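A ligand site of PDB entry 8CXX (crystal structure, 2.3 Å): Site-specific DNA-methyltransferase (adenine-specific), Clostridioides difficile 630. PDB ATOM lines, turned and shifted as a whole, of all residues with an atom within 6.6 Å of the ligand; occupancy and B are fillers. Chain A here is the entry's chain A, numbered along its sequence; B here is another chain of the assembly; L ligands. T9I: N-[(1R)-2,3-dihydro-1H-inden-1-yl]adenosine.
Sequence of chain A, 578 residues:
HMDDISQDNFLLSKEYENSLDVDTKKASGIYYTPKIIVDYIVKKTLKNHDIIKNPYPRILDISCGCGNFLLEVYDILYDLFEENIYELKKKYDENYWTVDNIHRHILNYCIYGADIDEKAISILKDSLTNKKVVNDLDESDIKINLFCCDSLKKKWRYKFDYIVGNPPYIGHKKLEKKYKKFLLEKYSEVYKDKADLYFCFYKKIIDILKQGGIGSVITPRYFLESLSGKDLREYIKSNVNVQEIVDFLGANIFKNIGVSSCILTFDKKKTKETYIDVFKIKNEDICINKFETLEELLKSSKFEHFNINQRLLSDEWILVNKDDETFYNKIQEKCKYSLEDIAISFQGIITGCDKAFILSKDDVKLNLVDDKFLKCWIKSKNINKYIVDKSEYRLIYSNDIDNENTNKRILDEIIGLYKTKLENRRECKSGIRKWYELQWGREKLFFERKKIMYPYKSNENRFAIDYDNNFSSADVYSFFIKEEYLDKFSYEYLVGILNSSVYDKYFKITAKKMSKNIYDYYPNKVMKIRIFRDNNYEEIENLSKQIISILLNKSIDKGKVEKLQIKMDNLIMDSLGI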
ATOM      1  N   GLY A  29     -18.800  -9.408 -28.978  1.00  0.00           N
ATOM      2  CA  GLY A  29     -17.605 -10.224 -29.108  1.00  0.00           C
ATOM      3  C   GLY A  29     -17.546 -11.408 -28.163  1.00  0.00           C
ATOM      4  O   GLY A  29     -16.703 -12.296 -28.316  1.00  0.00           O
ATOM      5  N   ILE A  30     -18.452 -11.423 -27.182  1.00  0.00           N
ATOM      6  CA  ILE A  30     -18.509 -12.467 -26.169  1.00  0.00           C
ATOM      7  C   ILE A  30     -19.857 -13.177 -26.269  1.00  0.00           C
ATOM      8  O   ILE A  30     -20.908 -12.525 -26.336  1.00  0.00           O
ATOM      9  CB  ILE A  30     -18.309 -11.901 -24.751  1.00  0.00           C
ATOM     10  N   TYR A  31     -19.833 -14.510 -26.297  1.00  0.00           N
ATOM     11  CA  TYR A  31     -21.024 -15.339 -26.470  1.00  0.00           C
ATOM     12  C   TYR A  31     -21.226 -16.224 -25.252  1.00  0.00           C
ATOM     13  O   TYR A  31     -20.280 -16.858 -24.762  1.00  0.00           O
ATOM     14  CB  TYR A  31     -20.899 -16.210 -27.723  1.00  0.00           C
ATOM     15  CG  TYR A  31     -20.809 -15.408 -29.007  1.00  0.00           C
ATOM     16  CD1 TYR A  31     -19.584 -14.963 -29.480  1.00  0.00           C
ATOM     17  CD2 TYR A  31     -21.949 -15.098 -29.726  1.00  0.00           C
ATOM     18  CE1 TYR A  31     -19.498 -14.212 -30.647  1.00  0.00           C
ATOM     19  CE2 TYR A  31     -21.880 -14.360 -30.895  1.00  0.00           C
ATOM     20  CZ  TYR A  31     -20.650 -13.925 -31.348  1.00  0.00           C
ATOM     21  OH  TYR A  31     -20.588 -13.187 -32.504  1.00  0.00           O
ATOM     22  N   ILE A  62      -9.224 -21.757 -23.365  1.00  0.00           N
ATOM     23  CA  ILE A  62      -8.350 -20.985 -24.247  1.00  0.00           C
ATOM     24  C   ILE A  62      -8.967 -19.660 -24.683  1.00  0.00           C
ATOM     25  O   ILE A  62      -8.244 -18.761 -25.116  1.00  0.00           O
ATOM     26  CB  ILE A  62      -7.986 -21.842 -25.465  1.00  0.00           C
ATOM     27  CG1 ILE A  62      -6.553 -21.573 -25.903  1.00  0.00           C
ATOM     28  CG2 ILE A  62      -8.935 -21.596 -26.595  1.00  0.00           C
ATOM     29  CD1 ILE A  62      -5.573 -22.105 -24.934  1.00  0.00           C
ATOM     30  N   SER A  63     -10.300 -19.527 -24.611  1.00  0.00           N
ATOM     31  CA  SER A  63     -10.968 -18.243 -24.779  1.00  0.00           C
ATOM     32  C   SER A  63     -12.092 -18.236 -23.743  1.00  0.00           C
ATOM     33  O   SER A  63     -13.241 -18.541 -24.057  1.00  0.00           O
ATOM     34  CB  SER A  63     -11.501 -18.067 -26.197  1.00  0.00           C
ATOM     35  OG  SER A  63     -12.346 -19.141 -26.527  1.00  0.00           O
ATOM     36  N   CYS A  64     -11.757 -17.816 -22.519  1.00  0.00           N
ATOM     37  CA  CYS A  64     -12.598 -18.091 -21.371  1.00  0.00           C
ATOM     38  C   CYS A  64     -13.703 -17.068 -21.161  1.00  0.00           C
ATOM     39  O   CYS A  64     -14.612 -17.346 -20.365  1.00  0.00           O
ATOM     40  CB  CYS A  64     -11.739 -18.172 -20.103  1.00  0.00           C
ATOM     41  SG  CYS A  64     -10.776 -16.678 -19.821  1.00  0.00           S
ATOM     42  N   GLY A  65     -13.653 -15.928 -21.843  1.00  0.00           N
ATOM     43  CA  GLY A  65     -14.694 -14.934 -21.664  1.00  0.00           C
ATOM     44  C   GLY A  65     -14.784 -14.494 -20.213  1.00  0.00           C
ATOM     45  O   GLY A  65     -13.774 -14.331 -19.518  1.00  0.00           O
ATOM     46  N   CYS A  66     -16.017 -14.332 -19.733  1.00  0.00           N
ATOM     47  CA  CYS A  66     -16.224 -13.968 -18.342  1.00  0.00           C
ATOM     48  C   CYS A  66     -16.045 -15.141 -17.383  1.00  0.00           C
ATOM     49  O   CYS A  66     -16.094 -14.949 -16.166  1.00  0.00           O
ATOM     50  CB  CYS A  66     -17.609 -13.353 -18.151  1.00  0.00           C
ATOM     51  SG  CYS A  66     -17.729 -11.658 -18.774  1.00  0.00           S
ATOM     52  N   ALA A 114      -7.355 -17.820 -20.813  1.00  0.00           N
ATOM     53  CA  ALA A 114      -6.826 -16.784 -21.695  1.00  0.00           C
ATOM     54  C   ALA A 114      -7.971 -16.197 -22.503  1.00  0.00           C
ATOM     55  O   ALA A 114      -8.864 -16.920 -22.942  1.00  0.00           O
ATOM     56  CB  ALA A 114      -5.755 -17.348 -22.635  1.00  0.00           C
ATOM     57  N   ASP A 115      -7.935 -14.882 -22.714  1.00  0.00           N
ATOM     58  CA  ASP A 115      -8.928 -14.228 -23.546  1.00  0.00           C
ATOM     59  C   ASP A 115      -8.392 -12.883 -24.009  1.00  0.00           C
ATOM     60  O   ASP A 115      -7.685 -12.202 -23.268  1.00  0.00           O
ATOM     61  CB  ASP A 115     -10.254 -14.040 -22.811  1.00  0.00           C
ATOM     62  CG  ASP A 115     -11.417 -13.796 -23.757  1.00  0.00           C
ATOM     63  OD1 ASP A 115     -11.439 -12.747 -24.438  1.00  0.00           O
ATOM     64  OD2 ASP A 115     -12.298 -14.687 -23.858  1.00  0.00           O
ATOM     65  N   ILE A 116      -8.737 -12.520 -25.242  1.00  0.00           N
ATOM     66  CA  ILE A 116      -8.263 -11.255 -25.801  1.00  0.00           C
ATOM     67  C   ILE A 116      -8.924 -10.055 -25.131  1.00  0.00           C
ATOM     68  O   ILE A 116      -8.360  -8.962 -25.152  1.00  0.00           O
ATOM     69  CB  ILE A 116      -8.489 -11.254 -27.332  1.00  0.00           C
ATOM     70  CG1 ILE A 116      -7.751 -10.078 -27.987  1.00  0.00           C
ATOM     71  CG2 ILE A 116      -9.972 -11.211 -27.664  1.00  0.00           C
ATOM     72  CD1 ILE A 116      -6.250 -10.084 -27.740  1.00  0.00           C
ATOM     73  N   ASP A 117     -10.095 -10.250 -24.518  1.00  0.00           N
ATOM     74  CA  ASP A 117     -10.891  -9.156 -23.966  1.00  0.00           C
ATOM     75  C   ASP A 117     -10.419  -8.856 -22.544  1.00  0.00           C
ATOM     76  O   ASP A 117     -10.653  -9.640 -21.620  1.00  0.00           O
ATOM     77  CB  ASP A 117     -12.369  -9.513 -23.996  1.00  0.00           C
ATOM     78  CG  ASP A 117     -13.253  -8.390 -23.457  1.00  0.00           C
ATOM     79  OD1 ASP A 117     -12.779  -7.248 -23.365  1.00  0.00           O
ATOM     80  OD2 ASP A 117     -14.420  -8.674 -23.129  1.00  0.00           O
ATOM     81  N   ALA A 120     -13.182  -8.704 -19.742  1.00  0.00           N
ATOM     82  CA  ALA A 120     -13.726 -10.001 -19.346  1.00  0.00           C
ATOM     83  C   ALA A 120     -12.789 -10.714 -18.384  1.00  0.00           C
ATOM     84  O   ALA A 120     -13.249 -11.330 -17.408  1.00  0.00           O
ATOM     85  CB  ALA A 120     -13.983 -10.858 -20.589  1.00  0.00           C
ATOM     86  N   CYS A 149      -4.512 -12.070 -23.871  1.00  0.00           N
ATOM     87  CA  CYS A 149      -3.602 -12.285 -24.979  1.00  0.00           C
ATOM     88  C   CYS A 149      -4.358 -12.934 -26.134  1.00  0.00           C
ATOM     89  O   CYS A 149      -5.512 -13.361 -25.975  1.00  0.00           O
ATOM     90  CB  CYS A 149      -2.425 -13.173 -24.578  1.00  0.00           C
ATOM     91  SG  CYS A 149      -2.925 -14.877 -24.274  1.00  0.00           S
ATOM     92  N   ASP A 150      -3.702 -13.010 -27.277  1.00  0.00           N
ATOM     93  CA  ASP A 150      -4.142 -13.844 -28.390  1.00  0.00           C
ATOM     94  C   ASP A 150      -3.653 -15.263 -28.141  1.00  0.00           C
ATOM     95  O   ASP A 150      -2.449 -15.536 -28.223  1.00  0.00           O
ATOM     96  CB  ASP A 150      -3.602 -13.287 -29.707  1.00  0.00           C
ATOM     97  CG  ASP A 150      -4.019 -14.121 -30.913  1.00  0.00           C
ATOM     98  OD1 ASP A 150      -4.659 -15.178 -30.748  1.00  0.00           O
ATOM     99  OD2 ASP A 150      -3.696 -13.702 -32.048  1.00  0.00           O
ATOM    100  N   SER A 151      -4.578 -16.172 -27.842  1.00  0.00           N
ATOM    101  CA  SER A 151      -4.195 -17.542 -27.496  1.00  0.00           C
ATOM    102  C   SER A 151      -3.466 -18.227 -28.652  1.00  0.00           C
ATOM    103  O   SER A 151      -2.680 -19.154 -28.413  1.00  0.00           O
ATOM    104  CB  SER A 151      -5.438 -18.349 -27.098  1.00  0.00           C
ATOM    105  OG  SER A 151      -6.050 -17.780 -25.962  1.00  0.00           O
ATOM    106  N   LEU A 152      -3.713 -17.787 -29.881  1.00  0.00           N
ATOM    107  CA  LEU A 152      -3.065 -18.379 -31.046  1.00  0.00           C
ATOM    108  C   LEU A 152      -1.618 -17.918 -31.198  1.00  0.00           C
ATOM    109  O   LEU A 152      -0.881 -18.514 -32.000  1.00  0.00           O
ATOM    110  CB  LEU A 152      -3.844 -18.055 -32.311  1.00  0.00           C
ATOM    111  CG  LEU A 152      -5.280 -18.572 -32.345  1.00  0.00           C
ATOM    112  CD1 LEU A 152      -5.883 -18.367 -33.719  1.00  0.00           C
ATOM    113  CD2 LEU A 152      -5.311 -20.044 -31.949  1.00  0.00           C
ATOM    114  N   LYS A 153      -1.201 -16.888 -30.469  1.00  0.00           N
ATOM    115  CA  LYS A 153       0.169 -16.411 -30.509  1.00  0.00           C
ATOM    116  C   LYS A 153       0.931 -16.632 -29.220  1.00  0.00           C
ATOM    117  O   LYS A 153       2.162 -16.539 -29.223  1.00  0.00           O
ATOM    118  CB  LYS A 153       0.194 -14.919 -30.860  1.00  0.00           C
ATOM    119  CG  LYS A 153      -0.241 -14.606 -32.274  1.00  0.00           C
ATOM    120  CD  LYS A 153      -0.129 -13.131 -32.573  1.00  0.00           C
ATOM    121  CE  LYS A 153      -0.483 -12.834 -34.017  1.00  0.00           C
ATOM    122  NZ  LYS A 153      -0.640 -11.381 -34.239  1.00  0.00           N
ATOM    123  N   ASN A 166     -15.406 -22.667 -25.450  1.00  0.00           N
ATOM    124  CA  ASN A 166     -16.122 -22.276 -26.659  1.00  0.00           C
ATOM    125  C   ASN A 166     -15.278 -21.246 -27.403  1.00  0.00           C
ATOM    126  O   ASN A 166     -15.271 -20.064 -27.018  1.00  0.00           O
ATOM    127  CB  ASN A 166     -17.494 -21.715 -26.311  1.00  0.00           C
ATOM    128  CG  ASN A 166     -18.303 -21.341 -27.535  1.00  0.00           C
ATOM    129  OD1 ASN A 166     -17.995 -21.755 -28.643  1.00  0.00           O
ATOM    130  ND2 ASN A 166     -19.348 -20.554 -27.327  1.00  0.00           N
ATOM    131  N   PRO A 167     -14.572 -21.658 -28.450  1.00  0.00           N
ATOM    132  CA  PRO A 167     -13.655 -20.731 -29.142  1.00  0.00           C
ATOM    133  C   PRO A 167     -14.406 -19.751 -30.022  1.00  0.00           C
ATOM    134  O   PRO A 167     -15.599 -19.943 -30.294  1.00  0.00           O
ATOM    135  CB  PRO A 167     -12.787 -21.683 -29.990  1.00  0.00           C
ATOM    136  CG  PRO A 167     -13.743 -22.793 -30.329  1.00  0.00           C
ATOM    137  CD  PRO A 167     -14.616 -22.983 -29.094  1.00  0.00           C
ATOM    138  N   PRO A 168     -13.756 -18.693 -30.484  1.00  0.00           N
ATOM    139  CA  PRO A 168     -14.413 -17.786 -31.444  1.00  0.00           C
ATOM    140  C   PRO A 168     -14.595 -18.448 -32.798  1.00  0.00           C
ATOM    141  O   PRO A 168     -13.754 -19.226 -33.245  1.00  0.00           O
ATOM    142  CB  PRO A 168     -13.452 -16.597 -31.523  1.00  0.00           C
ATOM    143  CG  PRO A 168     -12.125 -17.162 -31.131  1.00  0.00           C
ATOM    144  CD  PRO A 168     -12.415 -18.211 -30.102  1.00  0.00           C
ATOM    145  N   TYR A 169     -15.715 -18.135 -33.443  1.00  0.00           N
ATOM    146  CA  TYR A 169     -15.995 -18.561 -34.814  1.00  0.00           C
ATOM    147  C   TYR A 169     -15.933 -17.321 -35.688  1.00  0.00           C
ATOM    148  O   TYR A 169     -16.762 -16.406 -35.536  1.00  0.00           O
ATOM    149  CB  TYR A 169     -17.362 -19.248 -34.964  1.00  0.00           C
ATOM    150  CG  TYR A 169     -17.922 -20.062 -33.802  1.00  0.00           C
ATOM    151  CD1 TYR A 169     -17.103 -20.674 -32.876  1.00  0.00           C
ATOM    152  CD2 TYR A 169     -19.295 -20.239 -33.666  1.00  0.00           C
ATOM    153  CE1 TYR A 169     -17.627 -21.428 -31.831  1.00  0.00           C
ATOM    154  CE2 TYR A 169     -19.834 -20.986 -32.644  1.00  0.00           C
ATOM    155  CZ  TYR A 169     -18.996 -21.578 -31.724  1.00  0.00           C
ATOM    156  OH  TYR A 169     -19.523 -22.312 -30.688  1.00  0.00           O
ATOM    157  N   ILE A 170     -14.974 -17.256 -36.602  1.00  0.00           N
ATOM    158  CA  ILE A 170     -14.891 -16.148 -37.554  1.00  0.00           C
ATOM    159  C   ILE A 170     -14.547 -16.711 -38.916  1.00  0.00           C
ATOM    160  O   ILE A 170     -13.490 -17.332 -39.092  1.00  0.00           O
ATOM    161  CB  ILE A 170     -13.866 -15.078 -37.132  1.00  0.00           C
ATOM    162  CG1 ILE A 170     -14.127 -14.618 -35.689  1.00  0.00           C
ATOM    163  CG2 ILE A 170     -13.935 -13.882 -38.066  1.00  0.00           C
ATOM    164  CD1 ILE A 170     -13.134 -13.618 -35.172  1.00  0.00           C
ATOM    165  N   LEU A 175     -13.060 -12.059 -41.039  1.00  0.00           N
ATOM    166  CA  LEU A 175     -11.731 -12.088 -40.444  1.00  0.00           C
ATOM    167  C   LEU A 175     -10.850 -11.041 -41.113  1.00  0.00           C
ATOM    168  O   LEU A 175     -10.769 -10.999 -42.343  1.00  0.00           O
ATOM    169  CB  LEU A 175     -11.108 -13.477 -40.570  1.00  0.00           C
ATOM    170  CG  LEU A 175      -9.881 -13.768 -39.711  1.00  0.00           C
ATOM    171  CD1 LEU A 175     -10.176 -13.488 -38.247  1.00  0.00           C
ATOM    172  CD2 LEU A 175      -9.412 -15.208 -39.893  1.00  0.00           C
ATOM    173  N   TYR A 179      -4.732 -10.432 -40.335  1.00  0.00           N
ATOM    174  CA  TYR A 179      -4.555 -11.588 -39.456  1.00  0.00           C
ATOM    175  C   TYR A 179      -4.466 -12.898 -40.230  1.00  0.00           C
ATOM    176  O   TYR A 179      -3.819 -13.833 -39.760  1.00  0.00           O
ATOM    177  CB  TYR A 179      -5.690 -11.654 -38.434  1.00  0.00           C
ATOM    178  CG  TYR A 179      -5.334 -12.567 -37.279  1.00  0.00           C
ATOM    179  CD1 TYR A 179      -4.631 -12.087 -36.191  1.00  0.00           C
ATOM    180  CD2 TYR A 179      -5.668 -13.908 -37.300  1.00  0.00           C
ATOM    181  CE1 TYR A 179      -4.283 -12.913 -35.135  1.00  0.00           C
ATOM    182  CE2 TYR A 179      -5.332 -14.747 -36.258  1.00  0.00           C
ATOM    183  CZ  TYR A 179      -4.640 -14.251 -35.184  1.00  0.00           C
ATOM    184  OH  TYR A 179      -4.308 -15.077 -34.144  1.00  0.00           O
ATOM    185  N   LEU A 183      -2.262 -16.704 -39.941  1.00  0.00           N
ATOM    186  CA  LEU A 183      -2.906 -18.021 -39.891  1.00  0.00           C
ATOM    187  C   LEU A 183      -2.479 -18.901 -41.052  1.00  0.00           C
ATOM    188  O   LEU A 183      -2.225 -20.091 -40.874  1.00  0.00           O
ATOM    189  CB  LEU A 183      -4.425 -17.859 -39.875  1.00  0.00           C
ATOM    190  CG  LEU A 183      -5.004 -17.250 -38.603  1.00  0.00           C
ATOM    191  CD1 LEU A 183      -6.504 -17.224 -38.681  1.00  0.00           C
ATOM    192  CD2 LEU A 183      -4.542 -18.036 -37.384  1.00  0.00           C
ATOM    193  N   LEU A 197     -11.629 -19.472 -38.301  1.00  0.00           N
ATOM    194  CA  LEU A 197     -10.721 -19.245 -37.181  1.00  0.00           C
ATOM    195  C   LEU A 197     -10.764 -20.383 -36.168  1.00  0.00           C
ATOM    196  O   LEU A 197      -9.742 -20.726 -35.566  1.00  0.00           O
ATOM    197  CB  LEU A 197     -11.046 -17.919 -36.496  1.00  0.00           C
ATOM    198  CG  LEU A 197     -10.189 -17.566 -35.282  1.00  0.00           C
ATOM    199  CD1 LEU A 197      -8.754 -17.324 -35.704  1.00  0.00           C
ATOM    200  CD2 LEU A 197     -10.749 -16.355 -34.561  1.00  0.00           C
ATOM    201  N   PHE A 201      -8.093 -22.959 -33.366  1.00  0.00           N
ATOM    202  CA  PHE A 201      -8.235 -23.252 -31.938  1.00  0.00           C
ATOM    203  C   PHE A 201      -8.254 -24.750 -31.687  1.00  0.00           C
ATOM    204  O   PHE A 201      -7.709 -25.221 -30.686  1.00  0.00           O
ATOM    205  CB  PHE A 201      -9.477 -22.564 -31.387  1.00  0.00           C
ATOM    206  CG  PHE A 201      -9.265 -21.121 -31.046  1.00  0.00           C
ATOM    207  CD1 PHE A 201      -9.210 -20.150 -32.045  1.00  0.00           C
ATOM    208  CD2 PHE A 201      -9.088 -20.715 -29.736  1.00  0.00           C
ATOM    209  CE1 PHE A 201      -8.997 -18.817 -31.736  1.00  0.00           C
ATOM    210  CE2 PHE A 201      -8.882 -19.382 -29.415  1.00  0.00           C
ATOM    211  CZ  PHE A 201      -8.840 -18.431 -30.421  1.00  0.00           C
ATOM    212  P    DA B   8     -20.952 -16.940 -40.220  1.00  0.00           P
ATOM    213  OP1  DA B   8     -21.281 -15.524 -40.476  1.00  0.00           O
ATOM    214  OP2  DA B   8     -19.540 -17.379 -40.206  1.00  0.00           O
ATOM    215  O5'  DA B   8     -21.665 -17.382 -38.865  1.00  0.00           O
ATOM    216  C5'  DA B   8     -20.953 -17.396 -37.641  1.00  0.00           C
ATOM    217  C4'  DA B   8     -21.922 -17.225 -36.499  1.00  0.00           C
ATOM    218  O4'  DA B   8     -21.378 -17.791 -35.285  1.00  0.00           O
ATOM    219  C3'  DA B   8     -22.287 -15.788 -36.169  1.00  0.00           C
ATOM    220  O3'  DA B   8     -23.673 -15.717 -35.903  1.00  0.00           O
ATOM    221  C2'  DA B   8     -21.465 -15.499 -34.910  1.00  0.00           C
ATOM    222  C1'  DA B   8     -21.530 -16.855 -34.237  1.00  0.00           C
ATOM    223  N9   DA B   8     -20.467 -17.097 -33.262  1.00  0.00           N
ATOM    224  C8   DA B   8     -19.161 -16.693 -33.352  1.00  0.00           C
ATOM    225  N7   DA B   8     -18.425 -17.070 -32.332  1.00  0.00           N
ATOM    226  C5   DA B   8     -19.307 -17.764 -31.518  1.00  0.00           C
ATOM    227  C6   DA B   8     -19.147 -18.418 -30.279  1.00  0.00           C
ATOM    228  N6   DA B   8     -17.980 -18.475 -29.625  1.00  0.00           N
ATOM    229  N1   DA B   8     -20.223 -19.022 -29.739  1.00  0.00           N
ATOM    230  C2   DA B   8     -21.398 -18.969 -30.398  1.00  0.00           C
ATOM    231  N3   DA B   8     -21.672 -18.386 -31.569  1.00  0.00           N
ATOM    232  C4   DA B   8     -20.569 -17.799 -32.079  1.00  0.00           C
HETATM  233  C7  T9I L   1     -10.117 -14.774 -27.969  1.00  0.00           C
HETATM  234  C5  T9I L   1     -11.545 -13.972 -29.413  1.00  0.00           C
HETATM  235  C4  T9I L   1     -12.496 -14.569 -27.131  1.00  0.00           C
HETATM  236  C3  T9I L   1     -15.531 -16.423 -27.494  1.00  0.00           C
HETATM  237  C2  T9I L   1     -14.465 -15.681 -26.711  1.00  0.00           C
HETATM  238  C1  T9I L   1     -13.563 -13.478 -27.139  1.00  0.00           C
HETATM  239  C6  T9I L   1      -9.507 -14.562 -29.197  1.00  0.00           C
HETATM  240  C10 T9I L   1      -7.909 -14.365 -31.705  1.00  0.00           C
HETATM  241  C18 T9I L   1      -7.264 -11.427 -33.803  1.00  0.00           C
HETATM  242  C11 T9I L   1      -7.362 -15.050 -32.971  1.00  0.00           C
HETATM  243  C12 T9I L   1      -7.695 -14.005 -34.042  1.00  0.00           C
HETATM  244  C13 T9I L   1      -7.511 -12.696 -33.310  1.00  0.00           C
HETATM  245  C17 T9I L   1      -7.161 -10.353 -32.917  1.00  0.00           C
HETATM  246  C14 T9I L   1      -7.643 -12.899 -31.948  1.00  0.00           C
HETATM  247  C16 T9I L   1      -7.302 -10.559 -31.559  1.00  0.00           C
HETATM  248  C15 T9I L   1      -7.548 -11.828 -31.066  1.00  0.00           C
HETATM  249  N   T9I L   1     -11.433 -14.416 -28.126  1.00  0.00           N
HETATM  250  C   T9I L   1     -14.742 -14.190 -26.454  1.00  0.00           C
HETATM  251  O   T9I L   1     -14.804 -13.922 -25.061  1.00  0.00           O
HETATM  252  C8  T9I L   1      -8.242 -15.534 -27.074  1.00  0.00           C
HETATM  253  C9  T9I L   1      -8.142 -14.915 -29.300  1.00  0.00           C
HETATM  254  N1  T9I L   1     -10.426 -14.037 -30.094  1.00  0.00           N
HETATM  255  N2  T9I L   1      -9.538 -15.255 -26.864  1.00  0.00           N
HETATM  256  N3  T9I L   1      -7.527 -15.399 -28.192  1.00  0.00           N
HETATM  257  N4  T9I L   1      -7.397 -14.863 -30.435  1.00  0.00           N
HETATM  258  O1  T9I L   1     -13.080 -12.358 -26.399  1.00  0.00           O
HETATM  259  O2  T9I L   1     -16.017 -15.648 -28.589  1.00  0.00           O
HETATM  260  O3  T9I L   1     -13.203 -15.755 -27.407  1.00  0.00           O
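OD2 of Asp 115 sits at hydrogen-bond distance from N of Cys 64 (3.4 Å).
The side-chain carboxylate (OD2) of Asp 150 lies within hydrogen-bond range of the side-chain hydroxyl (OH) of Tyr 179, 2.6 Å away.
The backbone NH of Leu 152 is in hydrogen-bond range of the side-chain carboxylate of Asp 150.
O of Ile 62 sits at hydrogen-bond distance from OG of Ser 151.
The backbone NH (N) of Ser 63 sits close to the backbone carbonyl oxygen (O) of Ala 114.
The backbone NH (N) of Ile 116 lies within hydrogen-bond range of the backbone carbonyl oxygen (O) of Cys 149, 3.4 Å away.
The backbone NH (N) of Tyr 169 is in hydrogen-bond range of N7 of DA 8 of chain B, at 3.1 Å.
OD1 of Asn 166 lies within hydrogen-bond range of OH of Tyr 169 (2.6 Å).
Residues that only touch the ligand: Ser 63 (3.1 Å), Tyr 179 (3.3 Å), Gly 65 (3.5 Å), DA 8 of chain B (3.6 Å), Cys 149 (3.6 Å), Pro 168 (3.7 Å), Asn 166 (3.7 Å), Leu 152 (3.7 Å), Tyr 31 (3.7 Å), Phe 201 (3.8 Å), Ile 62 (3.8 Å), Asp 117 (3.8 Å) and Leu 197 (3.8 Å).
Within 4 Å of the ligand: Gly 29, Tyr 31, Ile 62, Ser 63, Gly 65, Asp 115, Ile 116, Asp 117, Cys 149, Asp 150, Ser 151, Leu 152, Asn 166, Pro 168, Tyr 179, Leu 197, Phe 201 and DA 8 of chain B.
OD1 of Asp 115 is in hydrogen-bond range of O1 of the ligand.
OD1 of Asp 150 lies within hydrogen-bond range of N4 of the ligand.
The backbone NH of Ser 151 sits at hydrogen-bond distance from a nitrogen (N3) of the ligand (3.1 Å).
The backbone NH (N) of Ile 116 sits at hydrogen-bond distance from a nitrogen (N2) of the ligand, at 3.3 Å.
The backbone carbonyl oxygen (O) of Gly 29 lies close to an oxygen (O2) of the ligand (3.4 Å).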
